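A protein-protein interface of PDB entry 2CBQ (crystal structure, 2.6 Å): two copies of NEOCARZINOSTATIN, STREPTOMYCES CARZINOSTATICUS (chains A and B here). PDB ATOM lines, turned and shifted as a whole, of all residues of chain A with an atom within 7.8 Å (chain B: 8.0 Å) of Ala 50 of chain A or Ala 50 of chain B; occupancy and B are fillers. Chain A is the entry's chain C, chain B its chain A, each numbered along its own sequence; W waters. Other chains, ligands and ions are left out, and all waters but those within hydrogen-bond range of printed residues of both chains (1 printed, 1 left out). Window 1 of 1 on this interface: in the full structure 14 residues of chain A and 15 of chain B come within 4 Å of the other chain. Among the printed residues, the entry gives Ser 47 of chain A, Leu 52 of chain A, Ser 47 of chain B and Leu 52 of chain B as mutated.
O of Pro 49 of chain A sits close to O of Pro 49 of chain B (3.0 Å).
The backbone carbonyl oxygen (O) of Phe 76 of chain A lies within hydrogen-bond range of the backbone NH (N) of Ser 47 of chain A. O of Phe 76 of chain B is in hydrogen-bond range of N of Ser 47 of chain B.
Pro 49 of chain A touches Ala 50 of chain B (O to N, 3.8 Å). Leu 52 of chain B touches Pro 49 of chain A (CD1 to CG, 3.6 Å). Ala 50 of chain A touches Pro 49 of chain B. O of Ala 50 of chain A touches CA of Ala 50 of chain B (3.4 Å). Leu 52 of chain A touches Pro 49 of chain B. CA of Ser 53 of chain A touches CZ of Phe 76 of chain B, 3.95 Å away. Phe 76 of chain A touches Ser 53 of chain B (CZ to CA, 3.9 Å).
Printed residues of chain B within 4 Å of Ala 50 of chain A: Pro 49 (3.98 Å) and Ala 50 (3.4 Å). Of the printed residues of chain B, Leu 52 of chain A touches Pro 49 (3.8 Å). Of the printed residues of chain B, Ser 53 of chain A touches Phe 76 (3.95 Å). Glu 74 of chain A touches none of the printed residues of chain B. Of the printed residues of chain B, Phe 76 of chain A touches Ser 53. Printed residues of chain A within 4 Å of Leu 52 of chain B: Pro 49. Printed residues of chain A within 4 Å of Ser 53 of chain B: Phe 76 (3.9 Å).
Hydrophobic or aromatic side chains of chain B within 4 Å of the printed part of chain A: Pro 49, Ala 50, Leu 52 and Phe 76. Along chain B the printed residues that touch a printed residue of chain A span positions 49 to 76. Hydrophobic or aromatic side chains of chain A that line the printed part of chain B: Pro 49, Ala 50, Leu 52 and Phe 76.
Pro 49 of chain A touches its own counterpart, Pro 49 of chain B. Pro 49 of chain A touches Ala 50 of chain B, and with the chains exchanged Ala 50 of chain A touches Pro 49 of chain B. Pro 49 of chain A touches Leu 52 of chain B, and with the chains exchanged Leu 52 of chain A touches Pro 49 of chain B. Ser 53 of chain A touches Phe 76 of chain B, and with the chains exchanged Phe 76 of chain A touches Ser 53 of chain B. Positions printed for both chains: 47, 48, 49, 50, 51, 52, 53, 67, 68, 70, 73, 74 and 76. Of the 8 pairs that touch across the chains among the printed residues, 8 have their exchanged pair printed and touching as well.
Water W1 bridges OE2 of Glu 74 of chain B (2.5 Å) and O of Leu 52 of chain A (3.3 Å).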
ATOM      1  N   SER A  47       5.783  14.307  32.086  1.00  0.00           N
ATOM      2  CA  SER A  47       6.463  14.437  30.802  1.00  0.00           C
ATOM      3  C   SER A  47       5.681  15.167  29.715  1.00  0.00           C
ATOM      4  O   SER A  47       4.506  15.496  29.888  1.00  0.00           O
ATOM      5  CB  SER A  47       6.850  13.048  30.296  1.00  0.00           C
ATOM      6  OG  SER A  47       7.613  12.366  31.274  1.00  0.00           O
ATOM      7  N   ASN A  48       6.362  15.410  28.597  1.00  0.00           N
ATOM      8  CA  ASN A  48       5.780  16.087  27.438  1.00  0.00           C
ATOM      9  C   ASN A  48       5.616  15.125  26.245  1.00  0.00           C
ATOM     10  O   ASN A  48       6.520  14.993  25.417  1.00  0.00           O
ATOM     11  CB  ASN A  48       6.663  17.269  27.024  1.00  0.00           C
ATOM     12  CG  ASN A  48       6.231  17.873  25.708  1.00  0.00           C
ATOM     13  OD1 ASN A  48       5.059  18.184  25.517  1.00  0.00           O
ATOM     14  ND2 ASN A  48       7.169  18.037  24.791  1.00  0.00           N
ATOM     15  N   PRO A  49       4.456  14.452  26.136  1.00  0.00           N
ATOM     16  CA  PRO A  49       4.181  13.506  25.049  1.00  0.00           C
ATOM     17  C   PRO A  49       4.108  14.143  23.661  1.00  0.00           C
ATOM     18  O   PRO A  49       4.384  13.491  22.654  1.00  0.00           O
ATOM     19  CB  PRO A  49       2.847  12.890  25.467  1.00  0.00           C
ATOM     20  CG  PRO A  49       2.169  14.036  26.130  1.00  0.00           C
ATOM     21  CD  PRO A  49       3.276  14.586  27.004  1.00  0.00           C
ATOM     22  N   ALA A  50       3.732  15.415  23.613  1.00  0.00           N
ATOM     23  CA  ALA A  50       3.619  16.117  22.346  1.00  0.00           C
ATOM     24  C   ALA A  50       4.891  15.994  21.497  1.00  0.00           C
ATOM     25  O   ALA A  50       4.815  15.768  20.288  1.00  0.00           O
ATOM     26  CB  ALA A  50       3.289  17.582  22.592  1.00  0.00           C
ATOM     27  N   ASP A  51       6.054  16.114  22.135  1.00  0.00           N
ATOM     28  CA  ASP A  51       7.332  16.039  21.422  1.00  0.00           C
ATOM     29  C   ASP A  51       8.173  14.794  21.729  1.00  0.00           C
ATOM     30  O   ASP A  51       9.344  14.702  21.352  1.00  0.00           O
ATOM     31  CB  ASP A  51       8.118  17.322  21.693  1.00  0.00           C
ATOM     32  CG  ASP A  51       7.337  18.567  21.284  1.00  0.00           C
ATOM     33  OD1 ASP A  51       7.035  18.691  20.076  1.00  0.00           O
ATOM     34  OD2 ASP A  51       7.010  19.405  22.156  1.00  0.00           O
ATOM     35  N   LEU A  52       7.548  13.842  22.408  1.00  0.00           N
ATOM     36  CA  LEU A  52       8.165  12.576  22.768  1.00  0.00           C
ATOM     37  C   LEU A  52       8.768  11.911  21.523  1.00  0.00           C
ATOM     38  O   LEU A  52       8.317  12.126  20.400  1.00  0.00           O
ATOM     39  CB  LEU A  52       7.087  11.680  23.406  1.00  0.00           C
ATOM     40  CG  LEU A  52       7.249  10.199  23.757  1.00  0.00           C
ATOM     41  CD1 LEU A  52       7.298   9.408  22.476  1.00  0.00           C
ATOM     42  CD2 LEU A  52       8.494   9.966  24.598  1.00  0.00           C
ATOM     43  N   SER A  53       9.811  11.117  21.728  1.00  0.00           N
ATOM     44  CA  SER A  53      10.464  10.406  20.640  1.00  0.00           C
ATOM     45  C   SER A  53      11.221   9.255  21.269  1.00  0.00           C
ATOM     46  O   SER A  53      11.131   9.046  22.477  1.00  0.00           O
ATOM     47  CB  SER A  53      11.428  11.319  19.888  1.00  0.00           C
ATOM     48  OG  SER A  53      12.121  10.587  18.891  1.00  0.00           O
ATOM     49  N   LEU A  67      15.641  15.924  19.695  1.00  0.00           N
ATOM     50  CA  LEU A  67      14.485  16.150  20.554  1.00  0.00           C
ATOM     51  C   LEU A  67      14.162  17.640  20.623  1.00  0.00           C
ATOM     52  O   LEU A  67      15.037  18.451  20.938  1.00  0.00           O
ATOM     53  CB  LEU A  67      14.771  15.650  21.968  1.00  0.00           C
ATOM     54  CG  LEU A  67      13.636  15.882  22.973  1.00  0.00           C
ATOM     55  CD1 LEU A  67      12.455  14.974  22.621  1.00  0.00           C
ATOM     56  CD2 LEU A  67      14.136  15.618  24.399  1.00  0.00           C
ATOM     57  N   THR A  68      12.919  18.012  20.325  1.00  0.00           N
ATOM     58  CA  THR A  68      12.537  19.420  20.412  1.00  0.00           C
ATOM     59  C   THR A  68      12.097  19.678  21.851  1.00  0.00           C
ATOM     60  O   THR A  68      11.304  18.909  22.388  1.00  0.00           O
ATOM     61  CB  THR A  68      11.359  19.766  19.484  1.00  0.00           C
ATOM     62  OG1 THR A  68      11.755  19.600  18.122  1.00  0.00           O
ATOM     63  CG2 THR A  68      10.922  21.211  19.699  1.00  0.00           C
ATOM     64  N   ARG A  70      10.556  22.321  25.052  1.00  0.00           N
ATOM     65  CA  ARG A  70       9.568  23.376  25.249  1.00  0.00           C
ATOM     66  C   ARG A  70       9.768  24.082  26.582  1.00  0.00           C
ATOM     67  O   ARG A  70      10.056  23.441  27.594  1.00  0.00           O
ATOM     68  CB  ARG A  70       8.155  22.780  25.221  1.00  0.00           C
ATOM     69  CG  ARG A  70       7.833  21.917  23.999  1.00  0.00           C
ATOM     70  CD  ARG A  70       7.655  22.746  22.738  1.00  0.00           C
ATOM     71  NE  ARG A  70       7.516  21.921  21.538  1.00  0.00           N
ATOM     72  CZ  ARG A  70       7.540  22.402  20.293  1.00  0.00           C
ATOM     73  NH1 ARG A  70       7.694  23.707  20.090  1.00  0.00           N
ATOM     74  NH2 ARG A  70       7.433  21.587  19.251  1.00  0.00           N
ATOM     75  N   PHE A  73       4.781  23.117  28.588  1.00  0.00           N
ATOM     76  CA  PHE A  73       4.064  22.019  27.938  1.00  0.00           C
ATOM     77  C   PHE A  73       3.027  21.390  28.872  1.00  0.00           C
ATOM     78  O   PHE A  73       3.033  21.636  30.085  1.00  0.00           O
ATOM     79  CB  PHE A  73       5.053  20.952  27.458  1.00  0.00           C
ATOM     80  CG  PHE A  73       5.823  20.289  28.566  1.00  0.00           C
ATOM     81  CD1 PHE A  73       5.271  19.225  29.279  1.00  0.00           C
ATOM     82  CD2 PHE A  73       7.097  20.735  28.908  1.00  0.00           C
ATOM     83  CE1 PHE A  73       5.972  18.615  30.312  1.00  0.00           C
ATOM     84  CE2 PHE A  73       7.806  20.130  29.943  1.00  0.00           C
ATOM     85  CZ  PHE A  73       7.243  19.067  30.645  1.00  0.00           C
ATOM     86  N   GLU A  74       2.133  20.589  28.289  1.00  0.00           N
ATOM     87  CA  GLU A  74       1.093  19.894  29.046  1.00  0.00           C
ATOM     88  C   GLU A  74       1.735  18.641  29.624  1.00  0.00           C
ATOM     89  O   GLU A  74       2.130  17.739  28.881  1.00  0.00           O
ATOM     90  CB  GLU A  74      -0.064  19.506  28.126  1.00  0.00           C
ATOM     91  CG  GLU A  74      -1.316  19.046  28.860  1.00  0.00           C
ATOM     92  CD  GLU A  74      -2.431  18.636  27.910  1.00  0.00           C
ATOM     93  OE1 GLU A  74      -3.600  18.536  28.355  1.00  0.00           O
ATOM     94  OE2 GLU A  74      -2.134  18.401  26.714  1.00  0.00           O
ATOM     95  N   PHE A  76       2.126  15.071  31.695  1.00  0.00           N
ATOM     96  CA  PHE A  76       1.412  13.833  31.971  1.00  0.00           C
ATOM     97  C   PHE A  76       2.250  12.937  32.876  1.00  0.00           C
ATOM     98  O   PHE A  76       3.464  12.843  32.713  1.00  0.00           O
ATOM     99  CB  PHE A  76       1.117  13.097  30.658  1.00  0.00           C
ATOM    100  CG  PHE A  76       0.041  13.733  29.835  1.00  0.00           C
ATOM    101  CD1 PHE A  76      -1.293  13.385  30.026  1.00  0.00           C
ATOM    102  CD2 PHE A  76       0.356  14.686  28.866  1.00  0.00           C
ATOM    103  CE1 PHE A  76      -2.307  13.979  29.259  1.00  0.00           C
ATOM    104  CE2 PHE A  76      -0.641  15.287  28.095  1.00  0.00           C
ATOM    105  CZ  PHE A  76      -1.981  14.932  28.290  1.00  0.00           C
ATOM    106  N   SER B  47       1.044   3.732  18.009  1.00  0.00           N
ATOM    107  CA  SER B  47       0.316   4.953  18.366  1.00  0.00           C
ATOM    108  C   SER B  47       0.984   6.272  17.991  1.00  0.00           C
ATOM    109  O   SER B  47       2.135   6.302  17.558  1.00  0.00           O
ATOM    110  CB  SER B  47       0.060   4.956  19.861  1.00  0.00           C
ATOM    111  OG  SER B  47      -0.093   3.629  20.308  1.00  0.00           O
ATOM    112  N   ASN B  48       0.239   7.357  18.199  1.00  0.00           N
ATOM    113  CA  ASN B  48       0.669   8.724  17.906  1.00  0.00           C
ATOM    114  C   ASN B  48       0.791   9.571  19.190  1.00  0.00           C
ATOM    115  O   ASN B  48      -0.147  10.254  19.586  1.00  0.00           O
ATOM    116  CB  ASN B  48      -0.339   9.358  16.938  1.00  0.00           C
ATOM    117  CG  ASN B  48      -0.010  10.797  16.603  1.00  0.00           C
ATOM    118  OD1 ASN B  48       1.160  11.162  16.451  1.00  0.00           O
ATOM    119  ND2 ASN B  48      -1.042  11.620  16.464  1.00  0.00           N
ATOM    120  N   PRO B  49       1.962   9.551  19.840  1.00  0.00           N
ATOM    121  CA  PRO B  49       2.142  10.326  21.067  1.00  0.00           C
ATOM    122  C   PRO B  49       2.032  11.828  20.845  1.00  0.00           C
ATOM    123  O   PRO B  49       1.659  12.567  21.755  1.00  0.00           O
ATOM    124  CB  PRO B  49       3.538   9.907  21.528  1.00  0.00           C
ATOM    125  CG  PRO B  49       4.259   9.759  20.232  1.00  0.00           C
ATOM    126  CD  PRO B  49       3.245   8.965  19.406  1.00  0.00           C
ATOM    127  N   ALA B  50       2.360  12.279  19.641  1.00  0.00           N
ATOM    128  CA  ALA B  50       2.303  13.706  19.319  1.00  0.00           C
ATOM    129  C   ALA B  50       0.980  14.376  19.704  1.00  0.00           C
ATOM    130  O   ALA B  50       0.985  15.472  20.269  1.00  0.00           O
ATOM    131  CB  ALA B  50       2.569  13.914  17.837  1.00  0.00           C
ATOM    132  N   ASP B  51      -0.144  13.719  19.408  1.00  0.00           N
ATOM    133  CA  ASP B  51      -1.459  14.277  19.716  1.00  0.00           C
ATOM    134  C   ASP B  51      -2.164  13.542  20.865  1.00  0.00           C
ATOM    135  O   ASP B  51      -3.339  13.782  21.164  1.00  0.00           O
ATOM    136  CB  ASP B  51      -2.338  14.258  18.466  1.00  0.00           C
ATOM    137  CG  ASP B  51      -1.760  15.087  17.331  1.00  0.00           C
ATOM    138  OD1 ASP B  51      -1.599  16.319  17.511  1.00  0.00           O
ATOM    139  OD2 ASP B  51      -1.466  14.506  16.259  1.00  0.00           O
ATOM    140  N   LEU B  52      -1.434  12.640  21.504  1.00  0.00           N
ATOM    141  CA  LEU B  52      -1.940  11.878  22.640  1.00  0.00           C
ATOM    142  C   LEU B  52      -2.607  12.823  23.647  1.00  0.00           C
ATOM    143  O   LEU B  52      -2.398  14.032  23.615  1.00  0.00           O
ATOM    144  CB  LEU B  52      -0.750  11.130  23.282  1.00  0.00           C
ATOM    145  CG  LEU B  52      -0.648  10.644  24.734  1.00  0.00           C
ATOM    146  CD1 LEU B  52      -0.637  11.834  25.692  1.00  0.00           C
ATOM    147  CD2 LEU B  52      -1.796   9.708  25.039  1.00  0.00           C
ATOM    148  N   SER B  53      -3.415  12.259  24.535  1.00  0.00           N
ATOM    149  CA  SER B  53      -4.101  13.019  25.580  1.00  0.00           C
ATOM    150  C   SER B  53      -4.678  11.992  26.551  1.00  0.00           C
ATOM    151  O   SER B  53      -4.471  10.800  26.370  1.00  0.00           O
ATOM    152  CB  SER B  53      -5.215  13.889  24.989  1.00  0.00           C
ATOM    153  OG  SER B  53      -5.900  14.587  26.015  1.00  0.00           O
ATOM    154  N   LEU B  67      -9.760  15.133  20.812  1.00  0.00           N
ATOM    155  CA  LEU B  67      -8.594  14.478  20.258  1.00  0.00           C
ATOM    156  C   LEU B  67      -8.408  14.940  18.822  1.00  0.00           C
ATOM    157  O   LEU B  67      -9.360  14.982  18.031  1.00  0.00           O
ATOM    158  CB  LEU B  67      -8.765  12.956  20.286  1.00  0.00           C
ATOM    159  CG  LEU B  67      -7.609  12.173  19.656  1.00  0.00           C
ATOM    160  CD1 LEU B  67      -6.323  12.475  20.404  1.00  0.00           C
ATOM    161  CD2 LEU B  67      -7.909  10.689  19.681  1.00  0.00           C
ATOM    162  N   THR B  68      -7.178  15.291  18.483  1.00  0.00           N
ATOM    163  CA  THR B  68      -6.889  15.718  17.133  1.00  0.00           C
ATOM    164  C   THR B  68      -6.305  14.529  16.375  1.00  0.00           C
ATOM    165  O   THR B  68      -5.191  14.097  16.661  1.00  0.00           O
ATOM    166  CB  THR B  68      -5.898  16.874  17.140  1.00  0.00           C
ATOM    167  OG1 THR B  68      -6.459  17.955  17.892  1.00  0.00           O
ATOM    168  CG2 THR B  68      -5.613  17.342  15.714  1.00  0.00           C
ATOM    169  N   ARG B  70      -5.081  12.313  12.859  1.00  0.00           N
ATOM    170  CA  ARG B  70      -4.273  12.556  11.672  1.00  0.00           C
ATOM    171  C   ARG B  70      -4.482  11.451  10.658  1.00  0.00           C
ATOM    172  O   ARG B  70      -4.665  10.291  11.034  1.00  0.00           O
ATOM    173  CB  ARG B  70      -2.790  12.575  12.046  1.00  0.00           C
ATOM    174  CG  ARG B  70      -2.442  13.462  13.221  1.00  0.00           C
ATOM    175  CD  ARG B  70      -2.514  14.915  12.825  1.00  0.00           C
ATOM    176  NE  ARG B  70      -2.306  15.803  13.962  1.00  0.00           N
ATOM    177  CZ  ARG B  70      -2.344  17.127  13.879  1.00  0.00           C
ATOM    178  NH1 ARG B  70      -2.582  17.699  12.705  1.00  0.00           N
ATOM    179  NH2 ARG B  70      -2.154  17.879  14.961  1.00  0.00           N
ATOM    180  N   PHE B  73       0.609   9.507  10.584  1.00  0.00           N
ATOM    181  CA  PHE B  73       1.358   9.890  11.784  1.00  0.00           C
ATOM    182  C   PHE B  73       2.564   9.000  12.079  1.00  0.00           C
ATOM    183  O   PHE B  73       2.612   7.853  11.648  1.00  0.00           O
ATOM    184  CB  PHE B  73       0.418   9.900  13.004  1.00  0.00           C
ATOM    185  CG  PHE B  73      -0.062   8.529  13.433  1.00  0.00           C
ATOM    186  CD1 PHE B  73       0.709   7.735  14.285  1.00  0.00           C
ATOM    187  CD2 PHE B  73      -1.296   8.039  12.998  1.00  0.00           C
ATOM    188  CE1 PHE B  73       0.260   6.478  14.699  1.00  0.00           C
ATOM    189  CE2 PHE B  73      -1.754   6.779  13.410  1.00  0.00           C
ATOM    190  CZ  PHE B  73      -0.972   6.001  14.263  1.00  0.00           C
ATOM    191  N   GLU B  74       3.535   9.538  12.814  1.00  0.00           N
ATOM    192  CA  GLU B  74       4.720   8.770  13.185  1.00  0.00           C
ATOM    193  C   GLU B  74       4.324   7.837  14.333  1.00  0.00           C
ATOM    194  O   GLU B  74       4.138   8.273  15.470  1.00  0.00           O
ATOM    195  CB  GLU B  74       5.827   9.702  13.655  1.00  0.00           C
ATOM    196  CG  GLU B  74       7.145   9.012  13.902  1.00  0.00           C
ATOM    197  CD  GLU B  74       8.092   9.872  14.716  1.00  0.00           C
ATOM    198  OE1 GLU B  74       9.324   9.687  14.599  1.00  0.00           O
ATOM    199  OE2 GLU B  74       7.604  10.730  15.485  1.00  0.00           O
ATOM    200  N   PHE B  76       4.576   4.782  17.148  1.00  0.00           N
ATOM    201  CA  PHE B  76       5.472   4.140  18.096  1.00  0.00           C
ATOM    202  C   PHE B  76       4.725   2.974  18.721  1.00  0.00           C
ATOM    203  O   PHE B  76       3.496   3.019  18.866  1.00  0.00           O
ATOM    204  CB  PHE B  76       5.859   5.117  19.206  1.00  0.00           C
ATOM    205  CG  PHE B  76       6.775   6.210  18.765  1.00  0.00           C
ATOM    206  CD1 PHE B  76       8.144   6.112  18.989  1.00  0.00           C
ATOM    207  CD2 PHE B  76       6.273   7.344  18.132  1.00  0.00           C
ATOM    208  CE1 PHE B  76       9.005   7.133  18.592  1.00  0.00           C
ATOM    209  CE2 PHE B  76       7.125   8.376  17.725  1.00  0.00           C
ATOM    210  CZ  PHE B  76       8.496   8.270  17.956  1.00  0.00           C
HETATM  211  O   HOH W   1       9.006  11.958  17.218  1.00  0.00           O
